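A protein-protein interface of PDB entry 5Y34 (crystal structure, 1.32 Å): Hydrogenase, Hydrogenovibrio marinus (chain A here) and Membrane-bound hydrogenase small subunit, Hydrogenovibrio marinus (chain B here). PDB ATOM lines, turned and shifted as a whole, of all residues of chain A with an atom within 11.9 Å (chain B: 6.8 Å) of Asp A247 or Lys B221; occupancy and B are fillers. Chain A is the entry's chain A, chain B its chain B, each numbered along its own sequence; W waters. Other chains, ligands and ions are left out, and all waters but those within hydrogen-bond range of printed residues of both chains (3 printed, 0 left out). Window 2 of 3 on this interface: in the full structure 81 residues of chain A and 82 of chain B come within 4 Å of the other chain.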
ATOM      1  N   PRO A 239       7.973 -32.077  12.822  1.00  0.00           N
ATOM      2  CA  PRO A 239       7.491 -30.835  13.463  1.00  0.00           C
ATOM      3  C   PRO A 239       7.133 -29.706  12.505  1.00  0.00           C
ATOM      4  O   PRO A 239       6.535 -28.698  12.884  1.00  0.00           O
ATOM      5  CB  PRO A 239       8.666 -30.402  14.357  1.00  0.00           C
ATOM      6  CG  PRO A 239       9.608 -31.554  14.402  1.00  0.00           C
ATOM      7  CD  PRO A 239       9.383 -32.357  13.152  1.00  0.00           C
ATOM      8  N   CYS A 240       7.558 -29.859  11.245  1.00  0.00           N
ATOM      9  CA  CYS A 240       7.441 -28.781  10.261  1.00  0.00           C
ATOM     10  C   CYS A 240       6.049 -28.738   9.639  1.00  0.00           C
ATOM     11  O   CYS A 240       5.803 -29.149   8.504  1.00  0.00           O
ATOM     12  CB  CYS A 240       8.559 -28.900   9.208  1.00  0.00           C
ATOM     13  SG  CYS A 240       8.682 -30.558   8.490  1.00  0.00           S
ATOM     14  N   ALA A 241       5.102 -28.218  10.424  1.00  0.00           N
ATOM     15  CA  ALA A 241       3.702 -28.148  10.007  1.00  0.00           C
ATOM     16  C   ALA A 241       3.528 -27.377   8.688  1.00  0.00           C
ATOM     17  O   ALA A 241       4.246 -26.395   8.434  1.00  0.00           O
ATOM     18  CB  ALA A 241       2.851 -27.521  11.120  1.00  0.00           C
ATOM     19  N   ILE A 242       2.526 -27.796   7.911  1.00  0.00           N
ATOM     20  CA  ILE A 242       2.300 -27.298   6.554  1.00  0.00           C
ATOM     21  C   ILE A 242       1.059 -26.416   6.526  1.00  0.00           C
ATOM     22  O   ILE A 242      -0.003 -26.799   7.031  1.00  0.00           O
ATOM     23  CB  ILE A 242       2.103 -28.468   5.548  1.00  0.00           C
ATOM     24  CG1 ILE A 242       3.376 -29.316   5.431  1.00  0.00           C
ATOM     25  CG2 ILE A 242       1.671 -27.959   4.176  1.00  0.00           C
ATOM     26  CD1 ILE A 242       3.145 -30.688   4.822  1.00  0.00           C
ATOM     27  N   ASN A 243       1.190 -25.239   5.925  1.00  0.00           N
ATOM     28  CA  ASN A 243       0.048 -24.350   5.714  1.00  0.00           C
ATOM     29  C   ASN A 243       0.340 -23.560   4.465  1.00  0.00           C
ATOM     30  O   ASN A 243       1.154 -22.635   4.488  1.00  0.00           O
ATOM     31  CB  ASN A 243      -0.097 -23.404   6.913  1.00  0.00           C
ATOM     32  CG  ASN A 243      -1.274 -22.440   6.799  1.00  0.00           C
ATOM     33  OD1 ASN A 243      -1.990 -22.394   5.794  1.00  0.00           O
ATOM     34  ND2 ASN A 243      -1.468 -21.640   7.850  1.00  0.00           N
ATOM     35  N   ILE A 244      -0.307 -23.934   3.370  1.00  0.00           N
ATOM     36  CA  ILE A 244       0.019 -23.276   2.103  1.00  0.00           C
ATOM     37  C   ILE A 244      -0.800 -22.022   1.825  1.00  0.00           C
ATOM     38  O   ILE A 244      -0.246 -21.003   1.356  1.00  0.00           O
ATOM     39  CB  ILE A 244      -0.024 -24.237   0.877  1.00  0.00           C
ATOM     40  CG1 ILE A 244       0.807 -25.500   1.137  1.00  0.00           C
ATOM     41  CG2 ILE A 244       0.452 -23.541  -0.407  1.00  0.00           C
ATOM     42  CD1 ILE A 244       2.227 -25.252   1.599  1.00  0.00           C
ATOM     43  N   ASP A 245      -2.092 -22.058   2.163  1.00  0.00           N
ATOM     44  CA  ASP A 245      -3.107 -21.129   1.685  1.00  0.00           C
ATOM     45  C   ASP A 245      -3.954 -20.510   2.809  1.00  0.00           C
ATOM     46  O   ASP A 245      -4.846 -19.737   2.514  1.00  0.00           O
ATOM     47  CB  ASP A 245      -4.033 -21.895   0.707  1.00  0.00           C
ATOM     48  CG  ASP A 245      -5.070 -21.000   0.024  1.00  0.00           C
ATOM     49  OD1 ASP A 245      -4.711 -19.912  -0.453  1.00  0.00           O
ATOM     50  OD2 ASP A 245      -6.258 -21.392  -0.062  1.00  0.00           O
ATOM     51  N   GLY A 246      -3.758 -20.954   4.050  1.00  0.00           N
ATOM     52  CA  GLY A 246      -4.635 -20.539   5.149  1.00  0.00           C
ATOM     53  C   GLY A 246      -4.092 -19.367   5.950  1.00  0.00           C
ATOM     54  O   GLY A 246      -2.995 -18.832   5.709  1.00  0.00           O
ATOM     55  N   ASP A 247      -4.892 -18.962   6.930  1.00  0.00           N
ATOM     56  CA  ASP A 247      -4.513 -17.933   7.873  1.00  0.00           C
ATOM     57  C   ASP A 247      -3.106 -18.179   8.429  1.00  0.00           C
ATOM     58  O   ASP A 247      -2.820 -19.282   8.909  1.00  0.00           O
ATOM     59  CB  ASP A 247      -5.531 -17.974   9.011  1.00  0.00           C
ATOM     60  CG  ASP A 247      -5.569 -16.708   9.822  1.00  0.00           C
ATOM     61  OD1 ASP A 247      -5.278 -15.624   9.279  1.00  0.00           O
ATOM     62  OD2 ASP A 247      -5.931 -16.803  11.010  1.00  0.00           O
ATOM     63  N   MET A 248      -2.260 -17.143   8.378  1.00  0.00           N
ATOM     64  CA  MET A 248      -0.899 -17.121   8.926  1.00  0.00           C
ATOM     65  C   MET A 248       0.070 -18.095   8.272  1.00  0.00           C
ATOM     66  O   MET A 248       1.088 -18.460   8.856  1.00  0.00           O
ATOM     67  CB  MET A 248      -0.891 -17.269  10.454  1.00  0.00           C
ATOM     68  CG  MET A 248      -1.445 -16.048  11.166  1.00  0.00           C
ATOM     69  SD  MET A 248      -0.993 -15.963  12.903  1.00  0.00           S
ATOM     70  CE  MET A 248      -1.614 -14.333  13.329  1.00  0.00           C
ATOM     71  N   ALA A 249      -0.224 -18.460   7.022  1.00  0.00           N
ATOM     72  CA  ALA A 249       0.655 -19.367   6.266  1.00  0.00           C
ATOM     73  C   ALA A 249       2.112 -18.915   6.247  1.00  0.00           C
ATOM     74  O   ALA A 249       3.016 -19.742   6.407  1.00  0.00           O
ATOM     75  CB  ALA A 249       0.133 -19.553   4.848  1.00  0.00           C
ATOM     76  N   ALA A 250       2.339 -17.605   6.107  1.00  0.00           N
ATOM     77  CA  ALA A 250       3.714 -17.084   6.073  1.00  0.00           C
ATOM     78  C   ALA A 250       4.504 -17.448   7.318  1.00  0.00           C
ATOM     79  O   ALA A 250       5.728 -17.545   7.273  1.00  0.00           O
ATOM     80  CB  ALA A 250       3.729 -15.584   5.844  1.00  0.00           C
ATOM     81  N   GLY A 251       3.796 -17.616   8.440  1.00  0.00           N
ATOM     82  CA  GLY A 251       4.431 -17.998   9.696  1.00  0.00           C
ATOM     83  C   GLY A 251       4.499 -19.489   9.987  1.00  0.00           C
ATOM     84  O   GLY A 251       5.050 -19.888  11.019  1.00  0.00           O
ATOM     85  N   ALA A 252       3.973 -20.323   9.082  1.00  0.00           N
ATOM     86  CA  ALA A 252       4.062 -21.777   9.259  1.00  0.00           C
ATOM     87  C   ALA A 252       5.445 -22.267   8.870  1.00  0.00           C
ATOM     88  O   ALA A 252       6.083 -21.655   8.002  1.00  0.00           O
ATOM     89  CB  ALA A 252       3.019 -22.496   8.432  1.00  0.00           C
ATOM     90  N   PRO A 253       5.903 -23.376   9.478  1.00  0.00           N
ATOM     91  CA  PRO A 253       7.173 -23.949   8.998  1.00  0.00           C
ATOM     92  C   PRO A 253       7.237 -24.183   7.479  1.00  0.00           C
ATOM     93  O   PRO A 253       8.248 -23.841   6.864  1.00  0.00           O
ATOM     94  CB  PRO A 253       7.271 -25.271   9.757  1.00  0.00           C
ATOM     95  CG  PRO A 253       6.572 -24.949  11.078  1.00  0.00           C
ATOM     96  CD  PRO A 253       5.396 -24.083  10.683  1.00  0.00           C
ATOM     97  N   ILE A 254       6.189 -24.753   6.889  1.00  0.00           N
ATOM     98  CA  ILE A 254       6.202 -25.080   5.459  1.00  0.00           C
ATOM     99  C   ILE A 254       5.039 -24.371   4.793  1.00  0.00           C
ATOM    100  O   ILE A 254       3.864 -24.589   5.129  1.00  0.00           O
ATOM    101  CB  ILE A 254       6.101 -26.599   5.235  1.00  0.00           C
ATOM    102  CG1 ILE A 254       7.269 -27.350   5.905  1.00  0.00           C
ATOM    103  CG2 ILE A 254       6.035 -26.925   3.745  1.00  0.00           C
ATOM    104  CD1 ILE A 254       8.671 -26.903   5.517  1.00  0.00           C
ATOM    105  N   ASN A 255       5.374 -23.471   3.891  1.00  0.00           N
ATOM    106  CA  ASN A 255       4.401 -22.710   3.124  1.00  0.00           C
ATOM    107  C   ASN A 255       4.860 -22.736   1.659  1.00  0.00           C
ATOM    108  O   ASN A 255       5.818 -23.446   1.325  1.00  0.00           O
ATOM    109  CB  ASN A 255       4.284 -21.286   3.672  1.00  0.00           C
ATOM    110  CG  ASN A 255       5.618 -20.587   3.765  1.00  0.00           C
ATOM    111  OD1 ASN A 255       6.390 -20.614   2.812  1.00  0.00           O
ATOM    112  ND2 ASN A 255       5.924 -20.000   4.896  1.00  0.00           N
ATOM    113  N   MET A 256       4.197 -21.970   0.796  1.00  0.00           N
ATOM    114  CA  MET A 256       4.517 -22.014  -0.637  1.00  0.00           C
ATOM    115  C   MET A 256       5.959 -21.626  -0.896  1.00  0.00           C
ATOM    116  O   MET A 256       6.623 -22.257  -1.731  1.00  0.00           O
ATOM    117  CB  MET A 256       3.609 -21.084  -1.439  1.00  0.00           C
ATOM    118  CG  MET A 256       3.777 -21.190  -2.959  1.00  0.00           C
ATOM    119  SD  MET A 256       2.970 -22.671  -3.574  1.00  0.00           S
ATOM    120  CE  MET A 256       4.347 -23.787  -3.808  1.00  0.00           C
ATOM    121  N   ARG A 258       8.583 -21.851   1.083  1.00  0.00           N
ATOM    122  CA  ARG A 258       9.509 -22.865   1.570  1.00  0.00           C
ATOM    123  C   ARG A 258       9.534 -24.066   0.619  1.00  0.00           C
ATOM    124  O   ARG A 258      10.606 -24.634   0.362  1.00  0.00           O
ATOM    125  CB  ARG A 258       9.101 -23.319   2.986  1.00  0.00           C
ATOM    126  CG  ARG A 258       9.166 -22.269   4.108  1.00  0.00           C
ATOM    127  CD  ARG A 258      10.591 -22.060   4.616  1.00  0.00           C
ATOM    128  NE  ARG A 258      11.303 -21.077   3.805  1.00  0.00           N
ATOM    129  CZ  ARG A 258      12.484 -20.573   4.130  1.00  0.00           C
ATOM    130  NH1 ARG A 258      13.038 -19.635   3.377  1.00  0.00           N
ATOM    131  NH2 ARG A 258      13.093 -20.987   5.226  1.00  0.00           N
ATOM    132  N   SER A 496      -2.427 -31.947   4.163  1.00  0.00           N
ATOM    133  CA  SER A 496      -1.297 -31.206   4.692  1.00  0.00           C
ATOM    134  C   SER A 496      -0.837 -31.728   6.063  1.00  0.00           C
ATOM    135  O   SER A 496       0.000 -31.093   6.714  1.00  0.00           O
ATOM    136  CB  SER A 496      -1.617 -29.715   4.799  1.00  0.00           C
ATOM    137  OG  SER A 496      -1.788 -29.120   3.534  1.00  0.00           O
ATOM    138  N   THR A 498       0.976 -33.638   9.188  1.00  0.00           N
ATOM    139  CA  THR A 498       2.377 -33.962   9.454  1.00  0.00           C
ATOM    140  C   THR A 498       2.640 -34.760  10.729  1.00  0.00           C
ATOM    141  O   THR A 498       3.751 -35.251  10.909  1.00  0.00           O
ATOM    142  CB  THR A 498       3.259 -32.695   9.505  1.00  0.00           C
ATOM    143  OG1 THR A 498       2.630 -31.694  10.337  1.00  0.00           O
ATOM    144  CG2 THR A 498       3.596 -32.161   8.091  1.00  0.00           C
ATOM    145  N   ARG B 201       8.377 -15.620  17.177  1.00  0.00           N
ATOM    146  CA  ARG B 201       7.109 -16.183  17.701  1.00  0.00           C
ATOM    147  C   ARG B 201       6.701 -15.569  19.058  1.00  0.00           C
ATOM    148  O   ARG B 201       5.626 -15.903  19.577  1.00  0.00           O
ATOM    149  CB  ARG B 201       7.131 -17.709  17.795  1.00  0.00           C
ATOM    150  CG  ARG B 201       7.379 -18.396  16.440  1.00  0.00           C
ATOM    151  CD  ARG B 201       7.073 -19.883  16.559  1.00  0.00           C
ATOM    152  NE  ARG B 201       7.318 -20.575  15.272  1.00  0.00           N
ATOM    153  CZ  ARG B 201       6.761 -21.728  14.907  1.00  0.00           C
ATOM    154  NH1 ARG B 201       7.081 -22.262  13.725  1.00  0.00           N
ATOM    155  NH2 ARG B 201       5.885 -22.376  15.659  1.00  0.00           N
ATOM    156  N   HIS B 204       3.095 -14.455  19.837  1.00  0.00           N
ATOM    157  CA  HIS B 204       2.181 -15.539  20.207  1.00  0.00           C
ATOM    158  C   HIS B 204       2.329 -15.936  21.671  1.00  0.00           C
ATOM    159  O   HIS B 204       1.318 -16.095  22.380  1.00  0.00           O
ATOM    160  CB  HIS B 204       2.372 -16.732  19.272  1.00  0.00           C
ATOM    161  CG  HIS B 204       2.046 -16.411  17.849  1.00  0.00           C
ATOM    162  ND1 HIS B 204       0.826 -15.904  17.474  1.00  0.00           N
ATOM    163  CD2 HIS B 204       2.773 -16.518  16.703  1.00  0.00           C
ATOM    164  CE1 HIS B 204       0.802 -15.715  16.171  1.00  0.00           C
ATOM    165  NE2 HIS B 204       1.974 -16.070  15.681  1.00  0.00           N
ATOM    166  N   ASP B 216      -1.405 -29.127  15.439  1.00  0.00           N
ATOM    167  CA  ASP B 216      -2.692 -28.497  15.683  1.00  0.00           C
ATOM    168  C   ASP B 216      -2.815 -27.163  14.943  1.00  0.00           C
ATOM    169  O   ASP B 216      -1.937 -26.782  14.171  1.00  0.00           O
ATOM    170  CB  ASP B 216      -2.978 -28.371  17.195  1.00  0.00           C
ATOM    171  CG  ASP B 216      -2.063 -27.384  17.918  1.00  0.00           C
ATOM    172  OD1 ASP B 216      -1.194 -26.726  17.313  1.00  0.00           O
ATOM    173  OD2 ASP B 216      -2.237 -27.256  19.163  1.00  0.00           O
ATOM    174  N   GLU B 217      -3.915 -26.456  15.170  1.00  0.00           N
ATOM    175  CA  GLU B 217      -4.132 -25.159  14.563  1.00  0.00           C
ATOM    176  C   GLU B 217      -2.951 -24.215  14.816  1.00  0.00           C
ATOM    177  O   GLU B 217      -2.452 -23.547  13.892  1.00  0.00           O
ATOM    178  CB  GLU B 217      -5.434 -24.550  15.094  1.00  0.00           C
ATOM    179  CG  GLU B 217      -5.687 -23.154  14.573  1.00  0.00           C
ATOM    180  CD  GLU B 217      -6.912 -22.496  15.171  1.00  0.00           C
ATOM    181  OE1 GLU B 217      -7.368 -21.514  14.555  1.00  0.00           O
ATOM    182  OE2 GLU B 217      -7.416 -22.938  16.234  1.00  0.00           O
ATOM    183  N   GLY B 218      -2.483 -24.178  16.067  1.00  0.00           N
ATOM    184  CA  GLY B 218      -1.376 -23.319  16.429  1.00  0.00           C
ATOM    185  C   GLY B 218      -0.110 -23.659  15.667  1.00  0.00           C
ATOM    186  O   GLY B 218       0.609 -22.754  15.221  1.00  0.00           O
ATOM    187  N   ALA B 219       0.187 -24.956  15.553  1.00  0.00           N
ATOM    188  CA  ALA B 219       1.388 -25.368  14.817  1.00  0.00           C
ATOM    189  C   ALA B 219       1.363 -24.836  13.387  1.00  0.00           C
ATOM    190  O   ALA B 219       2.385 -24.373  12.874  1.00  0.00           O
ATOM    191  CB  ALA B 219       1.528 -26.876  14.810  1.00  0.00           C
ATOM    192  N   ARG B 220       0.198 -24.906  12.752  1.00  0.00           N
ATOM    193  CA  ARG B 220       0.061 -24.493  11.353  1.00  0.00           C
ATOM    194  C   ARG B 220       0.054 -22.978  11.178  1.00  0.00           C
ATOM    195  O   ARG B 220       0.154 -22.475  10.065  1.00  0.00           O
ATOM    196  CB  ARG B 220      -1.190 -25.118  10.758  1.00  0.00           C
ATOM    197  CG  ARG B 220      -1.086 -26.628  10.686  1.00  0.00           C
ATOM    198  CD  ARG B 220      -2.401 -27.232  10.267  1.00  0.00           C
ATOM    199  NE  ARG B 220      -2.295 -28.684  10.206  1.00  0.00           N
ATOM    200  CZ  ARG B 220      -3.196 -29.478   9.650  1.00  0.00           C
ATOM    201  NH1 ARG B 220      -4.290 -28.960   9.097  1.00  0.00           N
ATOM    202  NH2 ARG B 220      -3.001 -30.794   9.660  1.00  0.00           N
ATOM    203  N   LYS B 221      -0.107 -22.251  12.289  1.00  0.00           N
ATOM    204  CA  LYS B 221      -0.014 -20.803  12.270  1.00  0.00           C
ATOM    205  C   LYS B 221       1.320 -20.275  12.784  1.00  0.00           C
ATOM    206  O   LYS B 221       1.545 -19.064  12.773  1.00  0.00           O
ATOM    207  CB  LYS B 221      -1.157 -20.190  13.102  1.00  0.00           C
ATOM    208  CG  LYS B 221      -2.542 -20.402  12.494  1.00  0.00           C
ATOM    209  CD  LYS B 221      -3.635 -19.771  13.347  1.00  0.00           C
ATOM    210  CE  LYS B 221      -5.006 -19.833  12.685  1.00  0.00           C
ATOM    211  NZ  LYS B 221      -6.034 -19.291  13.615  1.00  0.00           N
ATOM    212  N   GLY B 222       2.208 -21.169  13.224  1.00  0.00           N
ATOM    213  CA  GLY B 222       3.474 -20.751  13.795  1.00  0.00           C
ATOM    214  C   GLY B 222       3.386 -20.157  15.195  1.00  0.00           C
ATOM    215  O   GLY B 222       4.164 -19.254  15.542  1.00  0.00           O
ATOM    216  N   TYR B 223       2.467 -20.680  16.006  1.00  0.00           N
ATOM    217  CA  TYR B 223       2.329 -20.238  17.393  1.00  0.00           C
ATOM    218  C   TYR B 223       3.537 -20.628  18.239  1.00  0.00           C
ATOM    219  O   TYR B 223       4.351 -21.458  17.860  1.00  0.00           O
ATOM    220  CB  TYR B 223       1.050 -20.813  18.007  1.00  0.00           C
ATOM    221  CG  TYR B 223      -0.252 -20.106  17.639  1.00  0.00           C
ATOM    222  CD1 TYR B 223      -0.308 -19.086  16.679  1.00  0.00           C
ATOM    223  CD2 TYR B 223      -1.439 -20.474  18.267  1.00  0.00           C
ATOM    224  CE1 TYR B 223      -1.512 -18.459  16.363  1.00  0.00           C
ATOM    225  CE2 TYR B 223      -2.644 -19.858  17.957  1.00  0.00           C
ATOM    226  CZ  TYR B 223      -2.683 -18.843  17.024  1.00  0.00           C
ATOM    227  OH  TYR B 223      -3.891 -18.242  16.722  1.00  0.00           O
HETATM  228  O   HOH W   1      -7.985 -18.863  11.421  1.00  0.00           O
HETATM  229  O   HOH W   2       7.616 -20.347  10.921  1.00  0.00           O
HETATM  230  O   HOH W   3      -3.784 -15.801  15.476  1.00  0.00           O
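The backbone carbonyl oxygen (O) of Arg B220 sits at hydrogen-bond distance from the side-chain amide nitrogen (ND2) of Asn A243.
NZ of Lys B221 is in salt-bridge range of OD2 of Asp A247 (3.6 Å).
The backbone carbonyl oxygen (O) of Ala A241 sits at hydrogen-bond distance from the backbone NH (N) of Ile A254 (3.0 Å).
N of Ala B219 lies within hydrogen-bond range of OD1 of Asp B216 (2.9 Å).
The guanidinium group of Arg B201 sits close to the backbone carbonyl oxygen of Gly B222, 3.4 Å away.
The guanidinium group (NH2) of Arg B201 is in hydrogen-bond range of the backbone carbonyl oxygen (O) of Tyr B223 (2.8 Å).
The side-chain amide oxygen (OD1) of Asn A243 sits at hydrogen-bond distance from the backbone NH (N) of Gly A246, at 2.9 Å.
ND2 of Asn A243 lies within hydrogen-bond range of O of Asp A247, at 2.9 Å.
O of Ala B219 touches CB of Ala A241, at 3.6 Å.
Ile A242 touches Arg B220.
His B204 touches Met A248 (CE1 to SD, 3.7 Å).
Lys B221 touches Met A248.
O of Gly A251 touches CA of Gly B222, at 3.3 Å.
Arg B220 touches Ala A252.
CG of Pro A253 touches NH1 of Arg B201 (3.8 Å).
CD of Pro A253 touches O of Ala B219 (3.7 Å).
No residue of chain A comes within 4 Å of Glu B217.
No residue of chain A comes within 4 Å of Gly B218.
Of chain A, only Ala A241 and Pro A253 come within 4 Å of Ala B219.
No residue of chain A comes within 4 Å of Tyr B223.
Of the printed residues of chain B, Ala A241 touches Ala B219 (3.6 Å).
Of the printed residues of chain A, His B204 touches Met A248.
Of the printed residues of chain B, Asn A243 touches Arg B220.
The nearest printed residue of chain A that does not touch Lys B221 is Gly A251 (4.01 Å).
Printed residues of chain A that touch a printed residue of chain B: Ala A241, Ile A242, Asn A243, Asp A247, Met A248, Gly A251, Ala A252 and Pro A253.
Hydrophobic or aromatic side chains of chain A within 4 Å of the printed part of chain B: Ala A241, Met A248, Ala A252 and Pro A253.
Of the 10 printed residues of chain B, 6 touch a printed residue of chain A.
Printed residues of chain B that touch a printed residue of chain A: Arg B201, His B204, Ala B219, Arg B220, Lys B221 and Gly B222.
Hydrophobic or aromatic side chains of chain B within 4 Å of the printed part of chain A: His B204 and Ala B219.
Among the printed residues, Asp or Glu carboxylates within 4 Å of a Lys or Arg side-chain nitrogen of the other chain: Asp A247 with Lys B221.
Water W2 lies within hydrogen-bond range of O of Gly A251 and NH1 of Arg B201.
Water W3 lies within hydrogen-bond range of the side-chain hydroxyl of Tyr B223 and the side-chain sulfur of Met A248.
Water W1 lies within hydrogen-bond range of OD2 of Asp A247 (2.9 Å) and NZ of Lys B221 (3.0 Å).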
